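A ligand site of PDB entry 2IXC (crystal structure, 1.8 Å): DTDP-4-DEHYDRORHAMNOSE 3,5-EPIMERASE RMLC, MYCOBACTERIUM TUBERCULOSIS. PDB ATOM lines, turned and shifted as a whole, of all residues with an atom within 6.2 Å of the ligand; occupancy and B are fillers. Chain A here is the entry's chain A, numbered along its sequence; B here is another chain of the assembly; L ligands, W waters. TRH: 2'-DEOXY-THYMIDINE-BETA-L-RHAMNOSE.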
ATOM      1  N   GLN A  47     -13.265 -10.004 -13.410  1.00  0.00           N
ATOM      2  CA  GLN A  47     -12.230 -10.307 -12.437  1.00  0.00           C
ATOM      3  C   GLN A  47     -12.243  -9.279 -11.313  1.00  0.00           C
ATOM      4  O   GLN A  47     -12.594  -8.118 -11.535  1.00  0.00           O
ATOM      5  CB  GLN A  47     -10.826 -10.310 -13.099  1.00  0.00           C
ATOM      6  CG  GLN A  47      -9.665 -10.638 -12.121  1.00  0.00           C
ATOM      7  CD  GLN A  47      -8.390 -11.206 -12.775  1.00  0.00           C
ATOM      8  OE1 GLN A  47      -7.277 -11.088 -12.213  1.00  0.00           O
ATOM      9  NE2 GLN A  47      -8.548 -11.848 -13.914  1.00  0.00           N
ATOM     10  N   ASN A  49      -9.545  -8.014  -8.193  1.00  0.00           N
ATOM     11  CA  ASN A  49      -8.210  -8.156  -7.640  1.00  0.00           C
ATOM     12  C   ASN A  49      -8.089  -7.442  -6.311  1.00  0.00           C
ATOM     13  O   ASN A  49      -8.884  -6.518  -5.994  1.00  0.00           O
ATOM     14  CB  ASN A  49      -7.150  -7.589  -8.605  1.00  0.00           C
ATOM     15  CG  ASN A  49      -6.948  -8.449  -9.836  1.00  0.00           C
ATOM     16  OD1 ASN A  49      -7.308  -9.627  -9.848  1.00  0.00           O
ATOM     17  ND2 ASN A  49      -6.366  -7.855 -10.889  1.00  0.00           N
ATOM     18  N   SER A  51      -4.831  -6.031  -3.514  1.00  0.00           N
ATOM     19  CA  SER A  51      -3.426  -5.897  -3.179  1.00  0.00           C
ATOM     20  C   SER A  51      -3.297  -5.236  -1.815  1.00  0.00           C
ATOM     21  O   SER A  51      -4.190  -4.487  -1.394  1.00  0.00           O
ATOM     22  CB  SER A  51      -2.671  -5.100  -4.232  1.00  0.00           C
ATOM     23  OG  SER A  51      -3.060  -3.730  -4.193  1.00  0.00           O
ATOM     24  N   ARG A  59       2.504   1.515  -7.070  1.00  0.00           N
ATOM     25  CA  ARG A  59       2.145   0.577  -8.124  1.00  0.00           C
ATOM     26  C   ARG A  59       1.622   1.360  -9.329  1.00  0.00           C
ATOM     27  O   ARG A  59       0.648   2.122  -9.212  1.00  0.00           O
ATOM     28  CB  ARG A  59       1.074  -0.399  -7.627  1.00  0.00           C
ATOM     29  CG  ARG A  59       1.509  -1.235  -6.405  1.00  0.00           C
ATOM     30  CD  ARG A  59       0.409  -2.230  -5.987  1.00  0.00           C
ATOM     31  NE  ARG A  59       0.744  -2.867  -4.713  1.00  0.00           N
ATOM     32  CZ  ARG A  59       1.021  -4.158  -4.571  1.00  0.00           C
ATOM     33  NH1 ARG A  59       0.966  -4.975  -5.635  1.00  0.00           N
ATOM     34  NH2 ARG A  59       1.336  -4.626  -3.368  1.00  0.00           N
ATOM     35  N   GLY A  60       2.266   1.190 -10.489  1.00  0.00           N
ATOM     36  CA  GLY A  60       1.853   1.882 -11.711  1.00  0.00           C
ATOM     37  C   GLY A  60       3.035   2.355 -12.560  1.00  0.00           C
ATOM     38  O   GLY A  60       4.178   2.045 -12.223  1.00  0.00           O
ATOM     39  N   LEU A  61       2.785   3.077 -13.655  1.00  0.00           N
ATOM     40  CA  LEU A  61       1.474   3.385 -14.214  1.00  0.00           C
ATOM     41  C   LEU A  61       1.061   2.276 -15.162  1.00  0.00           C
ATOM     42  O   LEU A  61       1.830   1.884 -16.044  1.00  0.00           O
ATOM     43  CB  LEU A  61       1.534   4.695 -14.988  1.00  0.00           C
ATOM     44  CG  LEU A  61       1.685   5.967 -14.144  1.00  0.00           C
ATOM     45  CD1 LEU A  61       2.053   7.204 -15.013  1.00  0.00           C
ATOM     46  CD2 LEU A  61       0.447   6.251 -13.302  1.00  0.00           C
ATOM     47  N   HIS A  62      -0.159   1.771 -14.996  1.00  0.00           N
ATOM     48  CA  HIS A  62      -0.583   0.574 -15.734  1.00  0.00           C
ATOM     49  C   HIS A  62      -1.763   0.813 -16.664  1.00  0.00           C
ATOM     50  O   HIS A  62      -2.668   1.567 -16.334  1.00  0.00           O
ATOM     51  CB  HIS A  62      -0.902  -0.569 -14.772  1.00  0.00           C
ATOM     52  CG  HIS A  62       0.251  -0.975 -13.915  1.00  0.00           C
ATOM     53  ND1 HIS A  62       0.089  -1.532 -12.670  1.00  0.00           N
ATOM     54  CD2 HIS A  62       1.585  -0.855 -14.117  1.00  0.00           C
ATOM     55  CE1 HIS A  62       1.278  -1.777 -12.139  1.00  0.00           C
ATOM     56  NE2 HIS A  62       2.207  -1.371 -12.994  1.00  0.00           N
ATOM     57  N   PHE A  63      -1.721   0.151 -17.820  1.00  0.00           N
ATOM     58  CA  PHE A  63      -2.862   0.167 -18.738  1.00  0.00           C
ATOM     59  C   PHE A  63      -2.976  -1.140 -19.511  1.00  0.00           C
ATOM     60  O   PHE A  63      -2.077  -1.967 -19.460  1.00  0.00           O
ATOM     61  CB  PHE A  63      -2.811   1.360 -19.697  1.00  0.00           C
ATOM     62  CG  PHE A  63      -1.747   1.257 -20.754  1.00  0.00           C
ATOM     63  CD1 PHE A  63      -2.090   0.873 -22.053  1.00  0.00           C
ATOM     64  CD2 PHE A  63      -0.419   1.550 -20.464  1.00  0.00           C
ATOM     65  CE1 PHE A  63      -1.103   0.775 -23.046  1.00  0.00           C
ATOM     66  CE2 PHE A  63       0.582   1.450 -21.441  1.00  0.00           C
ATOM     67  CZ  PHE A  63       0.235   1.056 -22.731  1.00  0.00           C
ATOM     68  N   GLN A  70      -9.182  -2.698 -20.108  1.00  0.00           N
ATOM     69  CA  GLN A  70      -9.670  -3.169 -18.817  1.00  0.00           C
ATOM     70  C   GLN A  70     -10.089  -1.964 -17.991  1.00  0.00           C
ATOM     71  O   GLN A  70      -9.227  -1.197 -17.498  1.00  0.00           O
ATOM     72  CB  GLN A  70      -8.562  -3.960 -18.102  1.00  0.00           C
ATOM     73  CG  GLN A  70      -8.972  -4.726 -16.836  1.00  0.00           C
ATOM     74  CD  GLN A  70      -7.772  -5.343 -16.092  1.00  0.00           C
ATOM     75  OE1 GLN A  70      -6.820  -4.639 -15.699  1.00  0.00           O
ATOM     76  NE2 GLN A  70      -7.835  -6.648 -15.867  1.00  0.00           N
ATOM     77  N   LYS A  72     -11.564  -0.372 -14.560  1.00  0.00           N
ATOM     78  CA  LYS A  72     -11.306  -0.706 -13.153  1.00  0.00           C
ATOM     79  C   LYS A  72     -12.148   0.179 -12.240  1.00  0.00           C
ATOM     80  O   LYS A  72     -12.193   1.398 -12.428  1.00  0.00           O
ATOM     81  CB  LYS A  72      -9.820  -0.516 -12.859  1.00  0.00           C
ATOM     82  CG  LYS A  72      -8.884  -1.377 -13.709  1.00  0.00           C
ATOM     83  CD  LYS A  72      -7.513  -0.673 -13.824  1.00  0.00           C
ATOM     84  CE  LYS A  72      -6.574  -1.364 -14.765  1.00  0.00           C
ATOM     85  NZ  LYS A  72      -5.206  -0.772 -14.650  1.00  0.00           N
ATOM     86  N   VAL A  74     -12.150   1.058  -8.415  1.00  0.00           N
ATOM     87  CA  VAL A  74     -11.075   0.889  -7.432  1.00  0.00           C
ATOM     88  C   VAL A  74     -11.355   1.607  -6.118  1.00  0.00           C
ATOM     89  O   VAL A  74     -11.761   2.753  -6.131  1.00  0.00           O
ATOM     90  CB  VAL A  74      -9.768   1.520  -7.990  1.00  0.00           C
ATOM     91  CG1 VAL A  74      -8.560   1.264  -7.075  1.00  0.00           C
ATOM     92  CG2 VAL A  74      -9.520   1.041  -9.458  1.00  0.00           C
ATOM     93  N   HIS A 119      -3.276   4.067 -14.881  1.00  0.00           N
ATOM     94  CA  HIS A 119      -3.671   4.169 -13.488  1.00  0.00           C
ATOM     95  C   HIS A 119      -2.534   3.736 -12.590  1.00  0.00           C
ATOM     96  O   HIS A 119      -1.744   2.834 -12.943  1.00  0.00           O
ATOM     97  CB  HIS A 119      -4.940   3.312 -13.252  1.00  0.00           C
ATOM     98  CG  HIS A 119      -5.332   3.158 -11.813  1.00  0.00           C
ATOM     99  ND1 HIS A 119      -5.232   1.967 -11.137  1.00  0.00           N
ATOM    100  CD2 HIS A 119      -5.855   4.044 -10.931  1.00  0.00           C
ATOM    101  CE1 HIS A 119      -5.658   2.116  -9.897  1.00  0.00           C
ATOM    102  NE2 HIS A 119      -6.051   3.363  -9.750  1.00  0.00           N
ATOM    103  N   GLY A 120      -2.426   4.397 -11.447  1.00  0.00           N
ATOM    104  CA  GLY A 120      -1.422   4.025 -10.454  1.00  0.00           C
ATOM    105  C   GLY A 120      -1.793   4.579  -9.091  1.00  0.00           C
ATOM    106  O   GLY A 120      -2.659   5.448  -8.980  1.00  0.00           O
ATOM    107  N   PHE A 121      -1.159   4.057  -8.044  1.00  0.00           N
ATOM    108  CA  PHE A 121      -1.313   4.655  -6.719  1.00  0.00           C
ATOM    109  C   PHE A 121      -0.054   4.552  -5.855  1.00  0.00           C
ATOM    110  O   PHE A 121       0.793   3.687  -6.093  1.00  0.00           O
ATOM    111  CB  PHE A 121      -2.524   4.096  -5.955  1.00  0.00           C
ATOM    112  CG  PHE A 121      -2.403   2.637  -5.622  1.00  0.00           C
ATOM    113  CD1 PHE A 121      -1.684   2.214  -4.502  1.00  0.00           C
ATOM    114  CD2 PHE A 121      -2.989   1.691  -6.452  1.00  0.00           C
ATOM    115  CE1 PHE A 121      -1.574   0.843  -4.192  1.00  0.00           C
ATOM    116  CE2 PHE A 121      -2.883   0.307  -6.146  1.00  0.00           C
ATOM    117  CZ  PHE A 121      -2.180  -0.112  -5.029  1.00  0.00           C
ATOM    118  N   TYR A 132     -10.233  -3.939  -6.562  1.00  0.00           N
ATOM    119  CA  TYR A 132     -10.782  -3.358  -7.766  1.00  0.00           C
ATOM    120  C   TYR A 132     -11.516  -4.351  -8.644  1.00  0.00           C
ATOM    121  O   TYR A 132     -11.031  -5.459  -8.858  1.00  0.00           O
ATOM    122  CB  TYR A 132      -9.752  -2.547  -8.550  1.00  0.00           C
ATOM    123  CG  TYR A 132      -8.500  -3.260  -8.998  1.00  0.00           C
ATOM    124  CD1 TYR A 132      -8.348  -3.659 -10.342  1.00  0.00           C
ATOM    125  CD2 TYR A 132      -7.443  -3.502  -8.102  1.00  0.00           C
ATOM    126  CE1 TYR A 132      -7.168  -4.304 -10.777  1.00  0.00           C
ATOM    127  CE2 TYR A 132      -6.277  -4.152  -8.538  1.00  0.00           C
ATOM    128  CZ  TYR A 132      -6.152  -4.536  -9.880  1.00  0.00           C
ATOM    129  OH  TYR A 132      -5.011  -5.201 -10.301  1.00  0.00           O
ATOM    130  N   CYS A 134     -12.767  -5.462 -12.291  1.00  0.00           N
ATOM    131  CA  CYS A 134     -12.148  -5.363 -13.626  1.00  0.00           C
ATOM    132  C   CYS A 134     -13.139  -5.787 -14.710  1.00  0.00           C
ATOM    133  O   CYS A 134     -13.865  -6.788 -14.534  1.00  0.00           O
ATOM    134  CB  CYS A 134     -10.922  -6.293 -13.727  1.00  0.00           C
ATOM    135  SG  CYS A 134      -9.599  -5.922 -12.572  1.00  0.00           S
ATOM    136  N   GLU A 137     -10.457 -10.124 -17.747  1.00  0.00           N
ATOM    137  CA  GLU A 137      -9.528 -10.966 -16.981  1.00  0.00           C
ATOM    138  C   GLU A 137      -8.076 -10.575 -17.270  1.00  0.00           C
ATOM    139  O   GLU A 137      -7.790  -9.987 -18.296  1.00  0.00           O
ATOM    140  CB  GLU A 137      -9.749 -12.435 -17.312  1.00  0.00           C
ATOM    141  CG  GLU A 137     -11.140 -12.970 -16.902  1.00  0.00           C
ATOM    142  CD  GLU A 137     -11.259 -14.471 -17.105  1.00  0.00           C
ATOM    143  OE1 GLU A 137     -11.472 -14.886 -18.258  1.00  0.00           O
ATOM    144  OE2 GLU A 137     -11.132 -15.216 -16.121  1.00  0.00           O
ATOM    145  N   TYR A 138      -7.180 -10.876 -16.334  1.00  0.00           N
ATOM    146  CA  TYR A 138      -5.736 -10.712 -16.498  1.00  0.00           C
ATOM    147  C   TYR A 138      -5.257 -11.182 -17.870  1.00  0.00           C
ATOM    148  O   TYR A 138      -5.595 -12.284 -18.307  1.00  0.00           O
ATOM    149  CB  TYR A 138      -5.068 -11.562 -15.423  1.00  0.00           C
ATOM    150  CG  TYR A 138      -3.565 -11.432 -15.295  1.00  0.00           C
ATOM    151  CD1 TYR A 138      -2.941 -10.201 -15.463  1.00  0.00           C
ATOM    152  CD2 TYR A 138      -2.791 -12.537 -14.937  1.00  0.00           C
ATOM    153  CE1 TYR A 138      -1.563 -10.077 -15.297  1.00  0.00           C
ATOM    154  CE2 TYR A 138      -1.417 -12.427 -14.776  1.00  0.00           C
ATOM    155  CZ  TYR A 138      -0.812 -11.203 -14.951  1.00  0.00           C
ATOM    156  OH  TYR A 138       0.552 -11.109 -14.757  1.00  0.00           O
ATOM    157  N   ASN A 139      -4.519 -10.303 -18.556  1.00  0.00           N
ATOM    158  CA  ASN A 139      -3.902 -10.609 -19.833  1.00  0.00           C
ATOM    159  C   ASN A 139      -2.524  -9.916 -19.836  1.00  0.00           C
ATOM    160  O   ASN A 139      -2.399  -8.763 -20.260  1.00  0.00           O
ATOM    161  CB  ASN A 139      -4.791 -10.133 -21.006  1.00  0.00           C
ATOM    162  CG  ASN A 139      -4.308 -10.640 -22.361  1.00  0.00           C
ATOM    163  OD1 ASN A 139      -3.125 -10.969 -22.541  1.00  0.00           O
ATOM    164  ND2 ASN A 139      -5.237 -10.704 -23.332  1.00  0.00           N
ATOM    165  N   GLU A 143      -1.368  -6.056 -21.129  1.00  0.00           N
ATOM    166  CA  GLU A 143      -1.211  -5.095 -20.044  1.00  0.00           C
ATOM    167  C   GLU A 143       0.232  -4.593 -19.988  1.00  0.00           C
ATOM    168  O   GLU A 143       1.172  -5.376 -20.023  1.00  0.00           O
ATOM    169  CB  GLU A 143      -1.592  -5.747 -18.707  1.00  0.00           C
ATOM    170  CG  GLU A 143      -3.092  -5.972 -18.549  1.00  0.00           C
ATOM    171  CD  GLU A 143      -3.459  -6.846 -17.333  1.00  0.00           C
ATOM    172  OE1 GLU A 143      -2.765  -6.771 -16.296  1.00  0.00           O
ATOM    173  OE2 GLU A 143      -4.451  -7.620 -17.459  1.00  0.00           O
ATOM    174  N   SER A 168       8.052  -2.370  -7.721  1.00  0.00           N
ATOM    175  CA  SER A 168       8.392  -3.720  -8.193  1.00  0.00           C
ATOM    176  C   SER A 168       9.508  -3.609  -9.236  1.00  0.00           C
ATOM    177  O   SER A 168       9.735  -2.548  -9.838  1.00  0.00           O
ATOM    178  CB  SER A 168       7.166  -4.370  -8.848  1.00  0.00           C
ATOM    179  OG  SER A 168       6.727  -3.586  -9.941  1.00  0.00           O
ATOM    180  N   ARG A 170       9.307  -4.813 -12.073  1.00  0.00           N
ATOM    181  CA  ARG A 170       8.539  -4.506 -13.288  1.00  0.00           C
ATOM    182  C   ARG A 170       8.365  -2.995 -13.448  1.00  0.00           C
ATOM    183  O   ARG A 170       8.704  -2.454 -14.509  1.00  0.00           O
ATOM    184  CB  ARG A 170       7.168  -5.179 -13.260  1.00  0.00           C
ATOM    185  CG  ARG A 170       6.316  -4.929 -14.515  1.00  0.00           C
ATOM    186  CD  ARG A 170       5.153  -5.885 -14.529  1.00  0.00           C
ATOM    187  NE  ARG A 170       4.218  -5.719 -15.642  1.00  0.00           N
ATOM    188  CZ  ARG A 170       3.109  -4.970 -15.588  1.00  0.00           C
ATOM    189  NH1 ARG A 170       2.304  -4.921 -16.638  1.00  0.00           N
ATOM    190  NH2 ARG A 170       2.798  -4.266 -14.494  1.00  0.00           N
ATOM    191  N   ASP A 171       7.844  -2.348 -12.415  1.00  0.00           N
ATOM    192  CA  ASP A 171       7.588  -0.896 -12.461  1.00  0.00           C
ATOM    193  C   ASP A 171       8.853  -0.031 -12.458  1.00  0.00           C
ATOM    194  O   ASP A 171       8.875   1.068 -13.049  1.00  0.00           O
ATOM    195  CB  ASP A 171       6.625  -0.484 -11.327  1.00  0.00           C
ATOM    196  CG  ASP A 171       5.186  -0.947 -11.604  1.00  0.00           C
ATOM    197  OD1 ASP A 171       4.879  -1.223 -12.778  1.00  0.00           O
ATOM    198  OD2 ASP A 171       4.377  -1.032 -10.650  1.00  0.00           O
ATOM    199  N   HIS B  19       0.269 -13.913  -4.019  1.00  0.00           N
ATOM    200  CA  HIS B  19       1.569 -13.571  -4.562  1.00  0.00           C
ATOM    201  C   HIS B  19       2.231 -12.567  -3.643  1.00  0.00           C
ATOM    202  O   HIS B  19       1.842 -11.390  -3.602  1.00  0.00           O
ATOM    203  CB  HIS B  19       1.423 -13.000  -5.975  1.00  0.00           C
ATOM    204  CG  HIS B  19       0.806 -13.950  -6.945  1.00  0.00           C
ATOM    205  ND1 HIS B  19       1.525 -14.952  -7.552  1.00  0.00           N
ATOM    206  CD2 HIS B  19      -0.475 -14.091  -7.367  1.00  0.00           C
ATOM    207  CE1 HIS B  19       0.716 -15.642  -8.342  1.00  0.00           C
ATOM    208  NE2 HIS B  19      -0.503 -15.139  -8.236  1.00  0.00           N
ATOM    209  N   ASP B  21       5.460 -10.324  -2.424  1.00  0.00           N
ATOM    210  CA  ASP B  21       6.687  -9.688  -2.875  1.00  0.00           C
ATOM    211  C   ASP B  21       7.157  -8.572  -1.923  1.00  0.00           C
ATOM    212  O   ASP B  21       6.588  -8.397  -0.829  1.00  0.00           O
ATOM    213  CB  ASP B  21       6.534  -9.185  -4.332  1.00  0.00           C
ATOM    214  CG  ASP B  21       5.568  -8.012  -4.463  1.00  0.00           C
ATOM    215  OD1 ASP B  21       5.184  -7.374  -3.457  1.00  0.00           O
ATOM    216  OD2 ASP B  21       5.175  -7.727  -5.618  1.00  0.00           O
ATOM    217  N   ARG B  23       6.675  -5.544  -1.866  1.00  0.00           N
ATOM    218  CA  ARG B  23       5.702  -4.485  -1.650  1.00  0.00           C
ATOM    219  C   ARG B  23       4.612  -4.845  -0.642  1.00  0.00           C
ATOM    220  O   ARG B  23       3.990  -3.960  -0.055  1.00  0.00           O
ATOM    221  CB  ARG B  23       5.057  -4.062  -2.974  1.00  0.00           C
ATOM    222  CG  ARG B  23       6.069  -3.496  -4.010  1.00  0.00           C
ATOM    223  CD  ARG B  23       5.444  -3.319  -5.391  1.00  0.00           C
ATOM    224  NE  ARG B  23       4.946  -4.588  -5.916  1.00  0.00           N
ATOM    225  CZ  ARG B  23       4.146  -4.723  -6.973  1.00  0.00           C
ATOM    226  NH1 ARG B  23       3.738  -3.660  -7.660  1.00  0.00           N
ATOM    227  NH2 ARG B  23       3.760  -5.941  -7.352  1.00  0.00           N
ATOM    228  N   PHE B  26      -0.472  -9.530  -3.517  1.00  0.00           N
ATOM    229  CA  PHE B  26      -1.495  -9.401  -4.551  1.00  0.00           C
ATOM    230  C   PHE B  26      -2.167 -10.756  -4.674  1.00  0.00           C
ATOM    231  O   PHE B  26      -1.482 -11.801  -4.595  1.00  0.00           O
ATOM    232  CB  PHE B  26      -0.859  -9.066  -5.910  1.00  0.00           C
ATOM    233  CG  PHE B  26      -1.878  -8.824  -7.007  1.00  0.00           C
ATOM    234  CD1 PHE B  26      -2.312  -7.534  -7.297  1.00  0.00           C
ATOM    235  CD2 PHE B  26      -2.444  -9.901  -7.701  1.00  0.00           C
ATOM    236  CE1 PHE B  26      -3.302  -7.323  -8.303  1.00  0.00           C
ATOM    237  CE2 PHE B  26      -3.406  -9.688  -8.689  1.00  0.00           C
ATOM    238  CZ  PHE B  26      -3.845  -8.407  -8.971  1.00  0.00           C
ATOM    239  N   PHE B  27      -3.495 -10.749  -4.851  1.00  0.00           N
ATOM    240  CA  PHE B  27      -4.222 -11.940  -5.266  1.00  0.00           C
ATOM    241  C   PHE B  27      -5.421 -11.620  -6.152  1.00  0.00           C
ATOM    242  O   PHE B  27      -6.039 -10.552  -6.016  1.00  0.00           O
ATOM    243  CB  PHE B  27      -4.624 -12.843  -4.077  1.00  0.00           C
ATOM    244  CG  PHE B  27      -5.610 -12.238  -3.122  1.00  0.00           C
ATOM    245  CD1 PHE B  27      -5.202 -11.306  -2.148  1.00  0.00           C
ATOM    246  CD2 PHE B  27      -6.947 -12.655  -3.142  1.00  0.00           C
ATOM    247  CE1 PHE B  27      -6.131 -10.789  -1.224  1.00  0.00           C
ATOM    248  CE2 PHE B  27      -7.892 -12.133  -2.221  1.00  0.00           C
ATOM    249  CZ  PHE B  27      -7.477 -11.195  -1.270  1.00  0.00           C
ATOM    250  N   GLU B  28      -5.715 -12.549  -7.041  1.00  0.00           N
ATOM    251  CA  GLU B  28      -6.903 -12.488  -7.858  1.00  0.00           C
ATOM    252  C   GLU B  28      -8.004 -13.081  -6.986  1.00  0.00           C
ATOM    253  O   GLU B  28      -8.013 -14.303  -6.709  1.00  0.00           O
ATOM    254  CB  GLU B  28      -6.696 -13.310  -9.154  1.00  0.00           C
ATOM    255  CG  GLU B  28      -5.453 -12.895  -9.969  1.00  0.00           C
ATOM    256  CD  GLU B  28      -5.215 -13.750 -11.218  1.00  0.00           C
ATOM    257  OE1 GLU B  28      -5.174 -14.995 -11.084  1.00  0.00           O
ATOM    258  OE2 GLU B  28      -5.038 -13.183 -12.324  1.00  0.00           O
HETATM  259  O4P TRH L   1       1.802  -3.743  -9.673  1.00  0.00           O
HETATM  260  P2  TRH L   1       0.442  -4.579  -9.539  1.00  0.00           P
HETATM  261  O3P TRH L   1      -0.423  -4.579  -8.203  1.00  0.00           O
HETATM  262  O1  TRH L   1      -0.527  -4.239 -10.813  1.00  0.00           O
HETATM  263  C1  TRH L   1      -1.776  -3.570 -10.698  1.00  0.00           C
HETATM  264  C2  TRH L   1      -2.570  -3.789 -11.998  1.00  0.00           C
HETATM  265  O2  TRH L   1      -1.720  -3.623 -13.141  1.00  0.00           O
HETATM  266  C3  TRH L   1      -3.716  -2.782 -12.103  1.00  0.00           C
HETATM  267  O3  TRH L   1      -4.302  -2.956 -13.391  1.00  0.00           O
HETATM  268  C4  TRH L   1      -3.253  -1.337 -11.893  1.00  0.00           C
HETATM  269  O4  TRH L   1      -4.396  -0.465 -11.945  1.00  0.00           O
HETATM  270  C5  TRH L   1      -2.513  -1.233 -10.558  1.00  0.00           C
HETATM  271  O5  TRH L   1      -1.448  -2.184 -10.555  1.00  0.00           O
HETATM  272  C6  TRH L   1      -1.917   0.153 -10.276  1.00  0.00           C
HETATM  273  OPP TRH L   1       0.691  -6.158  -9.844  1.00  0.00           O
HETATM  274  P   TRH L   1       1.914  -6.773 -10.698  1.00  0.00           P
HETATM  275  O1P TRH L   1       3.350  -6.311 -10.137  1.00  0.00           O
HETATM  276  O2P TRH L   1       1.561  -6.593 -12.254  1.00  0.00           O
HETATM  277  O5' TRH L   1       1.768  -8.331 -10.314  1.00  0.00           O
HETATM  278  C5' TRH L   1       1.935  -8.771  -8.958  1.00  0.00           C
HETATM  279  C4' TRH L   1       1.638 -10.280  -8.909  1.00  0.00           C
HETATM  280  O4' TRH L   1       0.236 -10.454  -9.197  1.00  0.00           O
HETATM  281  C3' TRH L   1       2.408 -11.105  -9.960  1.00  0.00           C
HETATM  282  O3' TRH L   1       2.876 -12.352  -9.384  1.00  0.00           O
HETATM  283  C2' TRH L   1       1.386 -11.377 -11.083  1.00  0.00           C
HETATM  284  C1' TRH L   1       0.052 -11.273 -10.363  1.00  0.00           C
HETATM  285  N11 TRH L   1      -1.104 -10.732 -11.076  1.00  0.00           N
HETATM  286  C21 TRH L   1      -2.157 -11.553 -11.351  1.00  0.00           C
HETATM  287  O21 TRH L   1      -2.115 -12.850 -11.051  1.00  0.00           O
HETATM  288  N31 TRH L   1      -3.261 -11.122 -11.968  1.00  0.00           N
HETATM  289  C41 TRH L   1      -3.355  -9.822 -12.282  1.00  0.00           C
HETATM  290  O41 TRH L   1      -4.459  -9.416 -12.870  1.00  0.00           O
HETATM  291  C51 TRH L   1      -2.318  -8.946 -12.022  1.00  0.00           C
HETATM  292  C5A TRH L   1      -2.453  -7.485 -12.414  1.00  0.00           C
HETATM  293  C61 TRH L   1      -1.174  -9.415 -11.392  1.00  0.00           C
HETATM  294  O   HOH W   1       4.414  -4.092 -11.217  1.00  0.00           O
HETATM  295  O   HOH W   2      -2.445  -3.941 -15.658  1.00  0.00           O
HETATM  296  O   HOH W   3       5.518  -7.730 -10.582  1.00  0.00           O
HETATM  297  O   HOH W   4       4.760 -11.711  -7.647  1.00  0.00           O
HETATM  298  O   HOH W   5       1.124  -8.618 -13.859  1.00  0.00           O
HETATM  299  O   HOH W   6       2.630  -9.548  -5.662  1.00  0.00           O
HETATM  300  O   HOH W   7      -4.770  -2.662 -16.571  1.00  0.00           O
HETATM  301  O   HOH W   8      -5.399  -5.169 -13.666  1.00  0.00           O
HETATM  302  O   HOH W   9       0.370  -5.019 -13.658  1.00  0.00           O
HETATM  303  O   HOH W  10      -5.382  -7.583 -14.496  1.00  0.00           O
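ND1 of His 62 is in hydrogen-bond range of O5 of the ligand.
NH2 of Arg 170 lies within salt-bridge range of O2P of the ligand, at 3.5 Å.
The guanidinium group (NH1) of Arg 23 of chain B lies within salt-bridge range of an oxygen (O4P) of the ligand (2.8 Å).
The side-chain amino group (NZ) of Lys 72 lies within hydrogen-bond range of an oxygen (O3) of the ligand, at 2.7 Å.
NH1 of Arg 59 lies within salt-bridge range of O3P of the ligand, 2.9 Å away.
The side-chain amide nitrogen (ND2) of Asn 49 lies within hydrogen-bond range of an oxygen (O41) of the ligand (3.2 Å).
An oxygen (O41) of the ligand lies close to the side-chain amide oxygen of Gln 47 (3.3 Å).
A ring nitrogen (ND1) of His 19 of chain B lies within hydrogen-bond range of an oxygen (O3') of the ligand (3.5 Å).
An oxygen (O4) of the ligand is in hydrogen-bond range of a ring nitrogen (ND1) of His 119 (2.7 Å).
N31 of the ligand sits at hydrogen-bond distance from OE2 of Glu 28 of chain B (2.7 Å).
The backbone NH (N) of Gly 60 is in hydrogen-bond range of the side-chain carboxylate (OD2) of Asp 171 (3.1 Å).
N of His 19 of chain B is in hydrogen-bond range of O of Phe 26 of chain B.
The side-chain carboxylate of Asp 21 of chain B lies within salt-bridge range of the guanidinium group of Arg 23 of chain B (2.9 Å).
OE2 of Glu 143 sits at hydrogen-bond distance from N of Asn 139 (2.9 Å).
O of Asn 49 sits at hydrogen-bond distance from N of Tyr 132.
N of Tyr 138 lies close to NE2 of Gln 47 (2.9 Å).
NH2 of Arg 170 lies within hydrogen-bond range of NE2 of His 62.
The backbone NH (N) of His 62 sits at hydrogen-bond distance from the backbone carbonyl oxygen (O) of His 119 (2.8 Å).
Gln 70 touches the ligand (OE1 to O3, 3.8 Å).
Gly 120 touches the ligand.
Tyr 132 touches the ligand (OH to C3, 3.3 Å).
CD1 of Tyr 138 touches O41 of the ligand, 3.1 Å away.
Glu 143 touches the ligand (OE1 to C5A, 3.96 Å).
Asp 171 touches the ligand.
Phe 26 of chain B touches the ligand.
Hydrophobic or aromatic side chains that line the ligand: His 62, His 119, Tyr 132, Tyr 138, His 19 of chain B and Phe 26 of chain B.
Of the 29 residues printed, 17 come within 4 Å of the ligand.
Along chain A the residues within 4 Å of the ligand span positions 47 to 171.
The nearest printed residue that does not touch the ligand is Phe 121 (4.2 Å).
Water W9 bridges O2P of the ligand and NH2 of Arg 170.
Water W10 lies within hydrogen-bond range of an oxygen (O41) of the ligand, the side-chain amide nitrogen (NE2) of Gln 70 and the side-chain carboxylate (OE2) of Glu 143.
Water W5 bridges an oxygen (O2P) of the ligand (2.6 Å) and the side-chain hydroxyl (OH) of Tyr 138 (2.7 Å).
Water W2 lies within hydrogen-bond range of an oxygen (O2) of the ligand and the side-chain carboxylate (OE1) of Glu 143.
Water W1 lies within hydrogen-bond range of an oxygen (O1P) of the ligand (2.7 Å), the side-chain hydroxyl (OG) of Ser 168 (2.7 Å) and the side-chain carboxylate (OD2) of Asp 171 (3.1 Å).
Water W6 lies within hydrogen-bond range of the backbone carbonyl oxygen of His 19 of chain B (2.9 Å) and the side-chain carboxylate of Asp 21 of chain B (3.1 Å).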
